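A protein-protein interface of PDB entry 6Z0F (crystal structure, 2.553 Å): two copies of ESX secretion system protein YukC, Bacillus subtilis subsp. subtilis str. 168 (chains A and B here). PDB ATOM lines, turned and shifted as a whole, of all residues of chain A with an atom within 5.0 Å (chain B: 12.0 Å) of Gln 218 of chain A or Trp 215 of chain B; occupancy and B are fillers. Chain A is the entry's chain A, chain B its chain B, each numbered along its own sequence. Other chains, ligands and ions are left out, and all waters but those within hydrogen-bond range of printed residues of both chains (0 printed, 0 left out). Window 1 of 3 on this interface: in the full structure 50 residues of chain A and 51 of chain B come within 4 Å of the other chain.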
ATOM      1  N   ILE A 208       5.272  24.850 -25.034  1.00  0.00           N
ATOM      2  CA  ILE A 208       4.623  25.104 -26.314  1.00  0.00           C
ATOM      3  C   ILE A 208       3.874  26.436 -26.173  1.00  0.00           C
ATOM      4  O   ILE A 208       3.437  26.791 -25.067  1.00  0.00           O
ATOM      5  CB  ILE A 208       3.712  23.901 -26.721  1.00  0.00           C
ATOM      6  CG1 ILE A 208       3.374  23.856 -28.225  1.00  0.00           C
ATOM      7  CG2 ILE A 208       2.456  23.840 -25.887  1.00  0.00           C
ATOM      8  CD1 ILE A 208       4.542  24.061 -29.176  1.00  0.00           C
ATOM      9  N   ILE A 210       0.761  28.432 -27.623  1.00  0.00           N
ATOM     10  CA  ILE A 210      -0.470  28.369 -28.396  1.00  0.00           C
ATOM     11  C   ILE A 210      -1.258  29.649 -28.198  1.00  0.00           C
ATOM     12  O   ILE A 210      -1.390  30.104 -27.061  1.00  0.00           O
ATOM     13  CB  ILE A 210      -1.307  27.147 -27.907  1.00  0.00           C
ATOM     14  CG1 ILE A 210      -0.521  25.861 -27.909  1.00  0.00           C
ATOM     15  CG2 ILE A 210      -2.556  26.957 -28.703  1.00  0.00           C
ATOM     16  CD1 ILE A 210      -0.979  24.923 -26.861  1.00  0.00           C
ATOM     17  N   LYS A 214      -6.977  29.549 -29.884  1.00  0.00           N
ATOM     18  CA  LYS A 214      -6.811  28.218 -30.460  1.00  0.00           C
ATOM     19  C   LYS A 214      -6.805  27.164 -29.358  1.00  0.00           C
ATOM     20  O   LYS A 214      -7.435  26.121 -29.501  1.00  0.00           O
ATOM     21  CB  LYS A 214      -5.523  28.130 -31.293  1.00  0.00           C
ATOM     22  N   TRP A 215      -6.114  27.452 -28.248  1.00  0.00           N
ATOM     23  CA  TRP A 215      -6.032  26.561 -27.095  1.00  0.00           C
ATOM     24  C   TRP A 215      -7.413  26.329 -26.498  1.00  0.00           C
ATOM     25  O   TRP A 215      -7.767  25.199 -26.173  1.00  0.00           O
ATOM     26  CB  TRP A 215      -5.099  27.178 -26.041  1.00  0.00           C
ATOM     27  CG  TRP A 215      -5.032  26.448 -24.730  1.00  0.00           C
ATOM     28  CD1 TRP A 215      -4.387  25.275 -24.481  1.00  0.00           C
ATOM     29  CD2 TRP A 215      -5.504  26.923 -23.461  1.00  0.00           C
ATOM     30  NE1 TRP A 215      -4.477  24.959 -23.145  1.00  0.00           N
ATOM     31  CE2 TRP A 215      -5.128  25.972 -22.491  1.00  0.00           C
ATOM     32  CE3 TRP A 215      -6.207  28.061 -23.049  1.00  0.00           C
ATOM     33  CZ2 TRP A 215      -5.472  26.104 -21.147  1.00  0.00           C
ATOM     34  CZ3 TRP A 215      -6.533  28.195 -21.715  1.00  0.00           C
ATOM     35  CH2 TRP A 215      -6.177  27.219 -20.784  1.00  0.00           C
ATOM     36  N   ASN A 216      -8.196  27.397 -26.374  1.00  0.00           N
ATOM     37  CA  ASN A 216      -9.517  27.320 -25.788  1.00  0.00           C
ATOM     38  C   ASN A 216     -10.492  26.569 -26.678  1.00  0.00           C
ATOM     39  O   ASN A 216     -11.327  25.851 -26.136  1.00  0.00           O
ATOM     40  CB  ASN A 216     -10.055  28.708 -25.481  1.00  0.00           C
ATOM     41  CG  ASN A 216      -9.856  29.110 -24.053  1.00  0.00           C
ATOM     42  OD1 ASN A 216     -10.075  28.320 -23.130  1.00  0.00           O
ATOM     43  ND2 ASN A 216      -9.453  30.350 -23.837  1.00  0.00           N
ATOM     44  N   ILE A 217     -10.412  26.710 -28.022  1.00  0.00           N
ATOM     45  CA  ILE A 217     -11.344  25.979 -28.893  1.00  0.00           C
ATOM     46  C   ILE A 217     -11.002  24.475 -28.845  1.00  0.00           C
ATOM     47  O   ILE A 217     -11.919  23.661 -28.779  1.00  0.00           O
ATOM     48  CB  ILE A 217     -11.474  26.532 -30.345  1.00  0.00           C
ATOM     49  CG1 ILE A 217     -12.604  25.828 -31.118  1.00  0.00           C
ATOM     50  CG2 ILE A 217     -10.177  26.472 -31.125  1.00  0.00           C
ATOM     51  CD1 ILE A 217     -13.995  25.905 -30.452  1.00  0.00           C
ATOM     52  N   GLN A 218      -9.709  24.113 -28.754  1.00  0.00           N
ATOM     53  CA  GLN A 218      -9.296  22.710 -28.658  1.00  0.00           C
ATOM     54  C   GLN A 218      -9.790  22.065 -27.352  1.00  0.00           C
ATOM     55  O   GLN A 218     -10.127  20.883 -27.342  1.00  0.00           O
ATOM     56  CB  GLN A 218      -7.769  22.586 -28.775  1.00  0.00           C
ATOM     57  CG  GLN A 218      -7.267  22.753 -30.204  1.00  0.00           C
ATOM     58  CD  GLN A 218      -5.761  22.741 -30.300  1.00  0.00           C
ATOM     59  OE1 GLN A 218      -5.127  21.694 -30.474  1.00  0.00           O
ATOM     60  NE2 GLN A 218      -5.154  23.913 -30.203  1.00  0.00           N
ATOM     61  N   ARG A 219      -9.883  22.857 -26.276  1.00  0.00           N
ATOM     62  CA  ARG A 219     -10.343  22.419 -24.963  1.00  0.00           C
ATOM     63  C   ARG A 219     -11.839  22.171 -24.964  1.00  0.00           C
ATOM     64  O   ARG A 219     -12.282  21.186 -24.376  1.00  0.00           O
ATOM     65  CB  ARG A 219      -9.998  23.458 -23.893  1.00  0.00           C
ATOM     66  CG  ARG A 219      -8.575  23.393 -23.408  1.00  0.00           C
ATOM     67  CD  ARG A 219      -8.223  24.675 -22.736  1.00  0.00           C
ATOM     68  NE  ARG A 219      -8.307  24.573 -21.280  1.00  0.00           N
ATOM     69  CZ  ARG A 219      -9.164  25.258 -20.532  1.00  0.00           C
ATOM     70  NH1 ARG A 219     -10.017  26.107 -21.094  1.00  0.00           N
ATOM     71  NH2 ARG A 219      -9.175  25.102 -19.215  1.00  0.00           N
ATOM     72  N   TYR A 220     -12.628  23.053 -25.617  1.00  0.00           N
ATOM     73  CA  TYR A 220     -14.076  22.838 -25.692  1.00  0.00           C
ATOM     74  C   TYR A 220     -14.375  21.684 -26.652  1.00  0.00           C
ATOM     75  O   TYR A 220     -15.361  20.998 -26.444  1.00  0.00           O
ATOM     76  CB  TYR A 220     -14.866  24.097 -26.087  1.00  0.00           C
ATOM     77  CG  TYR A 220     -14.546  25.324 -25.262  1.00  0.00           C
ATOM     78  CD1 TYR A 220     -14.165  25.214 -23.930  1.00  0.00           C
ATOM     79  CD2 TYR A 220     -14.619  26.596 -25.814  1.00  0.00           C
ATOM     80  CE1 TYR A 220     -13.827  26.336 -23.180  1.00  0.00           C
ATOM     81  CE2 TYR A 220     -14.294  27.726 -25.072  1.00  0.00           C
ATOM     82  CZ  TYR A 220     -13.900  27.593 -23.753  1.00  0.00           C
ATOM     83  OH  TYR A 220     -13.578  28.711 -23.015  1.00  0.00           O
ATOM     84  N   ILE A 221     -13.525  21.440 -27.675  1.00  0.00           N
ATOM     85  CA  ILE A 221     -13.687  20.304 -28.582  1.00  0.00           C
ATOM     86  C   ILE A 221     -13.492  19.021 -27.774  1.00  0.00           C
ATOM     87  O   ILE A 221     -14.346  18.141 -27.816  1.00  0.00           O
ATOM     88  CB  ILE A 221     -12.712  20.391 -29.790  1.00  0.00           C
ATOM     89  CG1 ILE A 221     -13.162  21.461 -30.792  1.00  0.00           C
ATOM     90  CG2 ILE A 221     -12.546  19.039 -30.492  1.00  0.00           C
ATOM     91  CD1 ILE A 221     -12.111  21.800 -31.837  1.00  0.00           C
ATOM     92  N   GLY A 222     -12.415  18.970 -26.995  1.00  0.00           N
ATOM     93  CA  GLY A 222     -12.099  17.833 -26.142  1.00  0.00           C
ATOM     94  C   GLY A 222     -13.148  17.569 -25.082  1.00  0.00           C
ATOM     95  O   GLY A 222     -13.515  16.416 -24.850  1.00  0.00           O
ATOM     96  N   THR B 206      -1.176  37.498 -26.309  1.00  0.00           N
ATOM     97  CA  THR B 206      -2.351  36.691 -26.632  1.00  0.00           C
ATOM     98  C   THR B 206      -2.073  35.176 -26.581  1.00  0.00           C
ATOM     99  O   THR B 206      -2.856  34.404 -27.123  1.00  0.00           O
ATOM    100  CB  THR B 206      -2.810  37.056 -28.041  1.00  0.00           C
ATOM    101  OG1 THR B 206      -1.786  36.698 -28.969  1.00  0.00           O
ATOM    102  CG2 THR B 206      -3.118  38.531 -28.185  1.00  0.00           C
ATOM    103  N   TYR B 207      -0.957  34.750 -25.986  1.00  0.00           N
ATOM    104  CA  TYR B 207      -0.566  33.349 -25.965  1.00  0.00           C
ATOM    105  C   TYR B 207      -0.565  32.770 -24.566  1.00  0.00           C
ATOM    106  O   TYR B 207      -0.283  33.475 -23.601  1.00  0.00           O
ATOM    107  CB  TYR B 207       0.848  33.188 -26.556  1.00  0.00           C
ATOM    108  CG  TYR B 207       0.897  33.001 -28.058  1.00  0.00           C
ATOM    109  CD1 TYR B 207       0.137  33.795 -28.903  1.00  0.00           C
ATOM    110  CD2 TYR B 207       1.758  32.079 -28.633  1.00  0.00           C
ATOM    111  CE1 TYR B 207       0.171  33.618 -30.281  1.00  0.00           C
ATOM    112  CE2 TYR B 207       1.830  31.920 -30.011  1.00  0.00           C
ATOM    113  CZ  TYR B 207       1.029  32.688 -30.835  1.00  0.00           C
ATOM    114  OH  TYR B 207       1.091  32.539 -32.202  1.00  0.00           O
ATOM    115  N   ILE B 208      -0.869  31.463 -24.470  1.00  0.00           N
ATOM    116  CA  ILE B 208      -0.799  30.677 -23.239  1.00  0.00           C
ATOM    117  C   ILE B 208       0.430  29.756 -23.361  1.00  0.00           C
ATOM    118  O   ILE B 208       0.793  29.348 -24.470  1.00  0.00           O
ATOM    119  CB  ILE B 208      -2.085  29.891 -22.927  1.00  0.00           C
ATOM    120  CG1 ILE B 208      -2.358  28.883 -24.007  1.00  0.00           C
ATOM    121  CG2 ILE B 208      -3.284  30.783 -22.648  1.00  0.00           C
ATOM    122  CD1 ILE B 208      -2.626  27.653 -23.495  1.00  0.00           C
ATOM    123  N   HIS B 209       1.072  29.433 -22.242  1.00  0.00           N
ATOM    124  CA  HIS B 209       2.290  28.628 -22.278  1.00  0.00           C
ATOM    125  C   HIS B 209       2.093  27.347 -21.488  1.00  0.00           C
ATOM    126  O   HIS B 209       1.994  27.374 -20.268  1.00  0.00           O
ATOM    127  CB  HIS B 209       3.482  29.461 -21.768  1.00  0.00           C
ATOM    128  CG  HIS B 209       3.569  30.802 -22.444  1.00  0.00           C
ATOM    129  ND1 HIS B 209       4.067  30.927 -23.728  1.00  0.00           N
ATOM    130  CD2 HIS B 209       3.115  32.009 -22.039  1.00  0.00           C
ATOM    131  CE1 HIS B 209       3.942  32.205 -24.045  1.00  0.00           C
ATOM    132  NE2 HIS B 209       3.373  32.896 -23.062  1.00  0.00           N
ATOM    133  N   ILE B 210       1.965  26.232 -22.203  1.00  0.00           N
ATOM    134  CA  ILE B 210       1.720  24.907 -21.621  1.00  0.00           C
ATOM    135  C   ILE B 210       2.956  24.057 -21.727  1.00  0.00           C
ATOM    136  O   ILE B 210       3.573  24.050 -22.787  1.00  0.00           O
ATOM    137  CB  ILE B 210       0.539  24.233 -22.374  1.00  0.00           C
ATOM    138  CG1 ILE B 210      -0.700  25.148 -22.383  1.00  0.00           C
ATOM    139  CG2 ILE B 210       0.212  22.810 -21.839  1.00  0.00           C
ATOM    140  CD1 ILE B 210      -1.192  25.537 -20.972  1.00  0.00           C
ATOM    141  N   PRO B 211       3.341  23.301 -20.676  1.00  0.00           N
ATOM    142  CA  PRO B 211       4.515  22.427 -20.811  1.00  0.00           C
ATOM    143  C   PRO B 211       4.244  21.376 -21.879  1.00  0.00           C
ATOM    144  O   PRO B 211       3.167  20.791 -21.883  1.00  0.00           O
ATOM    145  CB  PRO B 211       4.671  21.807 -19.416  1.00  0.00           C
ATOM    146  CG  PRO B 211       3.795  22.601 -18.513  1.00  0.00           C
ATOM    147  CD  PRO B 211       2.702  23.156 -19.357  1.00  0.00           C
ATOM    148  N   ARG B 212       5.179  21.191 -22.818  1.00  0.00           N
ATOM    149  CA  ARG B 212       5.054  20.262 -23.941  1.00  0.00           C
ATOM    150  C   ARG B 212       4.614  18.861 -23.511  1.00  0.00           C
ATOM    151  O   ARG B 212       3.838  18.236 -24.224  1.00  0.00           O
ATOM    152  CB  ARG B 212       6.377  20.177 -24.722  1.00  0.00           C
ATOM    153  CG  ARG B 212       6.227  19.512 -26.083  1.00  0.00           C
ATOM    154  CD  ARG B 212       7.501  19.562 -26.893  1.00  0.00           C
ATOM    155  NE  ARG B 212       7.416  20.528 -27.992  1.00  0.00           N
ATOM    156  CZ  ARG B 212       7.884  21.772 -27.936  1.00  0.00           C
ATOM    157  NH1 ARG B 212       8.483  22.215 -26.837  1.00  0.00           N
ATOM    158  NH2 ARG B 212       7.761  22.580 -28.981  1.00  0.00           N
ATOM    159  N   LYS B 213       5.059  18.386 -22.339  1.00  0.00           N
ATOM    160  CA  LYS B 213       4.653  17.072 -21.834  1.00  0.00           C
ATOM    161  C   LYS B 213       3.165  17.054 -21.481  1.00  0.00           C
ATOM    162  O   LYS B 213       2.480  16.084 -21.797  1.00  0.00           O
ATOM    163  CB  LYS B 213       5.486  16.669 -20.608  1.00  0.00           C
ATOM    164  N   LYS B 214       2.660  18.123 -20.843  1.00  0.00           N
ATOM    165  CA  LYS B 214       1.250  18.206 -20.481  1.00  0.00           C
ATOM    166  C   LYS B 214       0.395  18.326 -21.729  1.00  0.00           C
ATOM    167  O   LYS B 214      -0.621  17.653 -21.831  1.00  0.00           O
ATOM    168  CB  LYS B 214       0.986  19.386 -19.535  1.00  0.00           C
ATOM    169  CG  LYS B 214      -0.417  19.370 -18.941  1.00  0.00           C
ATOM    170  CD  LYS B 214      -0.584  20.413 -17.846  1.00  0.00           C
ATOM    171  CE  LYS B 214      -1.986  20.440 -17.289  1.00  0.00           C
ATOM    172  NZ  LYS B 214      -2.946  21.055 -18.244  1.00  0.00           N
ATOM    173  N   TRP B 215       0.820  19.145 -22.691  1.00  0.00           N
ATOM    174  CA  TRP B 215       0.075  19.343 -23.927  1.00  0.00           C
ATOM    175  C   TRP B 215       0.068  18.074 -24.778  1.00  0.00           C
ATOM    176  O   TRP B 215      -0.943  17.787 -25.410  1.00  0.00           O
ATOM    177  CB  TRP B 215       0.645  20.535 -24.717  1.00  0.00           C
ATOM    178  CG  TRP B 215      -0.124  20.909 -25.951  1.00  0.00           C
ATOM    179  CD1 TRP B 215       0.336  20.904 -27.233  1.00  0.00           C
ATOM    180  CD2 TRP B 215      -1.478  21.377 -26.012  1.00  0.00           C
ATOM    181  NE1 TRP B 215      -0.648  21.333 -28.091  1.00  0.00           N
ATOM    182  CE2 TRP B 215      -1.775  21.624 -27.367  1.00  0.00           C
ATOM    183  CE3 TRP B 215      -2.480  21.585 -25.057  1.00  0.00           C
ATOM    184  CZ2 TRP B 215      -3.030  22.064 -27.785  1.00  0.00           C
ATOM    185  CZ3 TRP B 215      -3.725  22.006 -25.476  1.00  0.00           C
ATOM    186  CH2 TRP B 215      -3.987  22.253 -26.823  1.00  0.00           C
ATOM    187  N   ASN B 216       1.159  17.289 -24.758  1.00  0.00           N
ATOM    188  CA  ASN B 216       1.233  16.044 -25.523  1.00  0.00           C
ATOM    189  C   ASN B 216       0.375  14.943 -24.916  1.00  0.00           C
ATOM    190  O   ASN B 216      -0.237  14.179 -25.662  1.00  0.00           O
ATOM    191  CB  ASN B 216       2.665  15.560 -25.658  1.00  0.00           C
ATOM    192  CG  ASN B 216       3.284  15.962 -26.967  1.00  0.00           C
ATOM    193  OD1 ASN B 216       2.654  15.877 -28.029  1.00  0.00           O
ATOM    194  ND2 ASN B 216       4.530  16.410 -26.921  1.00  0.00           N
ATOM    195  N   ILE B 217       0.308  14.872 -23.577  1.00  0.00           N
ATOM    196  CA  ILE B 217      -0.492  13.861 -22.894  1.00  0.00           C
ATOM    197  C   ILE B 217      -1.973  14.078 -23.210  1.00  0.00           C
ATOM    198  O   ILE B 217      -2.637  13.115 -23.588  1.00  0.00           O
ATOM    199  CB  ILE B 217      -0.201  13.846 -21.370  1.00  0.00           C
ATOM    200  CG1 ILE B 217       1.141  13.155 -21.090  1.00  0.00           C
ATOM    201  CG2 ILE B 217      -1.319  13.181 -20.563  1.00  0.00           C
ATOM    202  CD1 ILE B 217       1.640  13.348 -19.689  1.00  0.00           C
ATOM    203  N   GLN B 218      -2.476  15.327 -23.120  1.00  0.00           N
ATOM    204  CA  GLN B 218      -3.891  15.571 -23.412  1.00  0.00           C
ATOM    205  C   GLN B 218      -4.211  15.459 -24.913  1.00  0.00           C
ATOM    206  O   GLN B 218      -5.365  15.215 -25.251  1.00  0.00           O
ATOM    207  CB  GLN B 218      -4.402  16.894 -22.833  1.00  0.00           C
ATOM    208  CG  GLN B 218      -3.502  18.096 -23.032  1.00  0.00           C
ATOM    209  CD  GLN B 218      -3.784  19.202 -22.032  1.00  0.00           C
ATOM    210  OE1 GLN B 218      -4.786  19.202 -21.305  1.00  0.00           O
ATOM    211  NE2 GLN B 218      -2.895  20.178 -21.969  1.00  0.00           N
ATOM    212  N   ARG B 219      -3.211  15.575 -25.803  1.00  0.00           N
ATOM    213  CA  ARG B 219      -3.434  15.365 -27.230  1.00  0.00           C
ATOM    214  C   ARG B 219      -3.667  13.885 -27.518  1.00  0.00           C
ATOM    215  O   ARG B 219      -4.551  13.558 -28.304  1.00  0.00           O
ATOM    216  CB  ARG B 219      -2.264  15.885 -28.059  1.00  0.00           C
ATOM    217  CG  ARG B 219      -2.316  17.387 -28.250  1.00  0.00           C
ATOM    218  CD  ARG B 219      -2.632  17.769 -29.683  1.00  0.00           C
ATOM    219  NE  ARG B 219      -2.695  19.217 -29.884  1.00  0.00           N
ATOM    220  CZ  ARG B 219      -1.689  19.956 -30.347  1.00  0.00           C
ATOM    221  NH1 ARG B 219      -0.524  19.393 -30.651  1.00  0.00           N
ATOM    222  NH2 ARG B 219      -1.839  21.266 -30.507  1.00  0.00           N
ATOM    223  N   TYR B 220      -2.889  12.992 -26.883  1.00  0.00           N
ATOM    224  CA  TYR B 220      -3.097  11.551 -27.076  1.00  0.00           C
ATOM    225  C   TYR B 220      -4.392  11.111 -26.373  1.00  0.00           C
ATOM    226  O   TYR B 220      -5.054  10.199 -26.859  1.00  0.00           O
ATOM    227  CB  TYR B 220      -1.899  10.702 -26.603  1.00  0.00           C
ATOM    228  CG  TYR B 220      -0.560  11.148 -27.149  1.00  0.00           C
ATOM    229  CD1 TYR B 220      -0.455  11.730 -28.406  1.00  0.00           C
ATOM    230  CD2 TYR B 220       0.603  10.996 -26.405  1.00  0.00           C
ATOM    231  CE1 TYR B 220       0.768  12.181 -28.893  1.00  0.00           C
ATOM    232  CE2 TYR B 220       1.833  11.430 -26.888  1.00  0.00           C
ATOM    233  CZ  TYR B 220       1.914  12.023 -28.133  1.00  0.00           C
ATOM    234  OH  TYR B 220       3.132  12.450 -28.608  1.00  0.00           O
ATOM    235  N   ILE B 221      -4.770  11.767 -25.256  1.00  0.00           N
ATOM    236  CA  ILE B 221      -6.021  11.488 -24.552  1.00  0.00           C
ATOM    237  C   ILE B 221      -7.178  11.875 -25.471  1.00  0.00           C
ATOM    238  O   ILE B 221      -8.078  11.074 -25.685  1.00  0.00           O
ATOM    239  CB  ILE B 221      -6.079  12.229 -23.186  1.00  0.00           C
ATOM    240  CG1 ILE B 221      -5.150  11.568 -22.155  1.00  0.00           C
ATOM    241  CG2 ILE B 221      -7.510  12.316 -22.644  1.00  0.00           C
ATOM    242  CD1 ILE B 221      -4.934  12.407 -20.910  1.00  0.00           C
ATOM    243  N   GLY B 222      -7.102  13.066 -26.052  1.00  0.00           N
ATOM    244  CA  GLY B 222      -8.100  13.582 -26.981  1.00  0.00           C
ATOM    245  C   GLY B 222      -8.235  12.740 -28.231  1.00  0.00           C
ATOM    246  O   GLY B 222      -9.350  12.481 -28.678  1.00  0.00           O
ATOM    247  N   LEU B 223      -7.110  12.275 -28.788  1.00  0.00           N
ATOM    248  CA  LEU B 223      -7.127  11.405 -29.967  1.00  0.00           C
ATOM    249  C   LEU B 223      -7.664   9.996 -29.608  1.00  0.00           C
ATOM    250  O   LEU B 223      -8.347   9.370 -30.415  1.00  0.00           O
ATOM    251  CB  LEU B 223      -5.738  11.323 -30.614  1.00  0.00           C
ATOM    252  CG  LEU B 223      -5.426  12.456 -31.610  1.00  0.00           C
ATOM    253  CD1 LEU B 223      -3.966  12.445 -32.025  1.00  0.00           C
ATOM    254  CD2 LEU B 223      -6.339  12.399 -32.833  1.00  0.00           C
ATOM    255  N   GLY B 224      -7.403   9.547 -28.385  1.00  0.00           N
ATOM    256  CA  GLY B 224      -7.930   8.286 -27.876  1.00  0.00           C
ATOM    257  C   GLY B 224      -9.439   8.346 -27.691  1.00  0.00           C
ATOM    258  O   GLY B 224     -10.135   7.343 -27.866  1.00  0.00           O
ATOM    259  N   LEU B 225      -9.963   9.532 -27.344  1.00  0.00           N
ATOM    260  CA  LEU B 225     -11.398   9.751 -27.206  1.00  0.00           C
ATOM    261  C   LEU B 225     -12.077   9.671 -28.562  1.00  0.00           C
ATOM    262  O   LEU B 225     -13.177   9.142 -28.647  1.00  0.00           O
ATOM    263  CB  LEU B 225     -11.683  11.119 -26.578  1.00  0.00           C
ATOM    264  CG  LEU B 225     -11.289  11.284 -25.127  1.00  0.00           C
ATOM    265  CD1 LEU B 225     -11.406  12.723 -24.699  1.00  0.00           C
ATOM    266  CD2 LEU B 225     -12.107  10.386 -24.238  1.00  0.00           C
ATOM    267  N   ILE B 226     -11.431  10.187 -29.624  1.00  0.00           N
ATOM    268  CA  ILE B 226     -11.985  10.171 -30.975  1.00  0.00           C
ATOM    269  C   ILE B 226     -12.028   8.744 -31.514  1.00  0.00           C
ATOM    270  O   ILE B 226     -13.064   8.331 -32.025  1.00  0.00           O
ATOM    271  CB  ILE B 226     -11.195  11.106 -31.912  1.00  0.00           C
ATOM    272  CG1 ILE B 226     -11.298  12.556 -31.432  1.00  0.00           C
ATOM    273  CG2 ILE B 226     -11.683  10.985 -33.348  1.00  0.00           C
ATOM    274  CD1 ILE B 226     -10.362  13.503 -32.122  1.00  0.00           C
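The backbone NH (N) of Ile 208 of chain B is in hydrogen-bond range of the backbone carbonyl oxygen (O) of Ile 210 of chain A.
O of Ile 210 of chain B lies within hydrogen-bond range of N of Ile 208 of chain A (2.9 Å).
OE1 of Gln 218 of chain A is in hydrogen-bond range of NH2 of Arg 219 of chain B (3.3 Å).
The backbone carbonyl oxygen (O) of Lys 214 of chain A lies within hydrogen-bond range of the side-chain amide nitrogen (NE2) of Gln 218 of chain A (3.3 Å).
O of Arg 212 of chain B lies close to ND2 of Asn 216 of chain B (3.3 Å).
The indole nitrogen (NE1) of Trp 215 of chain B lies close to the guanidinium group (NH2) of Arg 219 of chain B (2.7 Å).
Among the printed residues, merely in contact across the chains: Ile 208 of chain A with Ile 208 of chain B, Ile 208 of chain A with His 209 of chain B, Ile 208 of chain A with Arg 212 of chain B, Ile 208 of chain A with Trp 215 of chain B, Ile 210 of chain A with Tyr 207 of chain B, Ile 210 of chain A with Trp 215 of chain B, Trp 215 of chain A with Ile 208 of chain B, Trp 215 of chain A with Ile 210 of chain B, Trp 215 of chain A with Trp 215 of chain B and Gln 218 of chain A with Trp 215 of chain B.
Of the printed residues of chain B, Gln 218 of chain A touches Trp 215 and Arg 219.
Of chain A, only Ile 208 (3.9 Å), Ile 210 (3.4 Å), Trp 215 (3.5 Å) and Gln 218 (3.4 Å) come within 4 Å of Trp 215 of chain B.
Ile 208 of chain A touches just these residues of chain B: Ile 208 (3.7 Å), His 209 (3.5 Å), Ile 210 (2.9 Å), Arg 212 (3.5 Å) and Trp 215 (3.9 Å).
Of chain B, only Tyr 207, Ile 208 and Trp 215 come within 4 Å of Ile 210 of chain A.
No residue of chain B comes within 4 Å of Lys 214 of chain A.
Trp 215 of chain A touches three residues of chain B.
No residue of chain B comes within 4 Å of Asn 216 of chain A.
No residue of chain B comes within 4 Å of Ile 221 of chain A.
No residue of chain B comes within 4 Å of Gly 222 of chain A.
Of the printed residues of chain A, Ile 210 of chain B touches Ile 208 (2.9 Å) and Trp 215 (3.9 Å).
Of the printed residues of chain A, Tyr 207 of chain B touches Ile 210.
The nearest residue of chain B that does not touch Gln 218 of chain A is Gly 222 of chain B (7.6 Å).
Of the 11 printed residues of chain A, 4 touch a printed residue of chain B.
Among the printed residues, no Asp or Glu carboxylate lies within 4 Å of a Lys or Arg side-chain nitrogen of the other chain.
Ile 208 of chain A touches Trp 215 of chain B, and with the chains exchanged Trp 215 of chain A touches Ile 208 of chain B.
Trp 215 of chain B touches its own counterpart, Trp 215 of chain A.
Gln 218 of chain A touches Trp 215 of chain B, but with the chains exchanged Trp 215 of chain A does not touch Gln 218 of chain B (5.2 Å).
Gln 218 of chain A touches Arg 219 of chain B, but with the chains exchanged Arg 219 of chain A does not touch Gln 218 of chain B (6.0 Å).
Of the 13 pairs that touch across the chains among the printed residues, 8 have their exchanged pair printed and touching as well.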
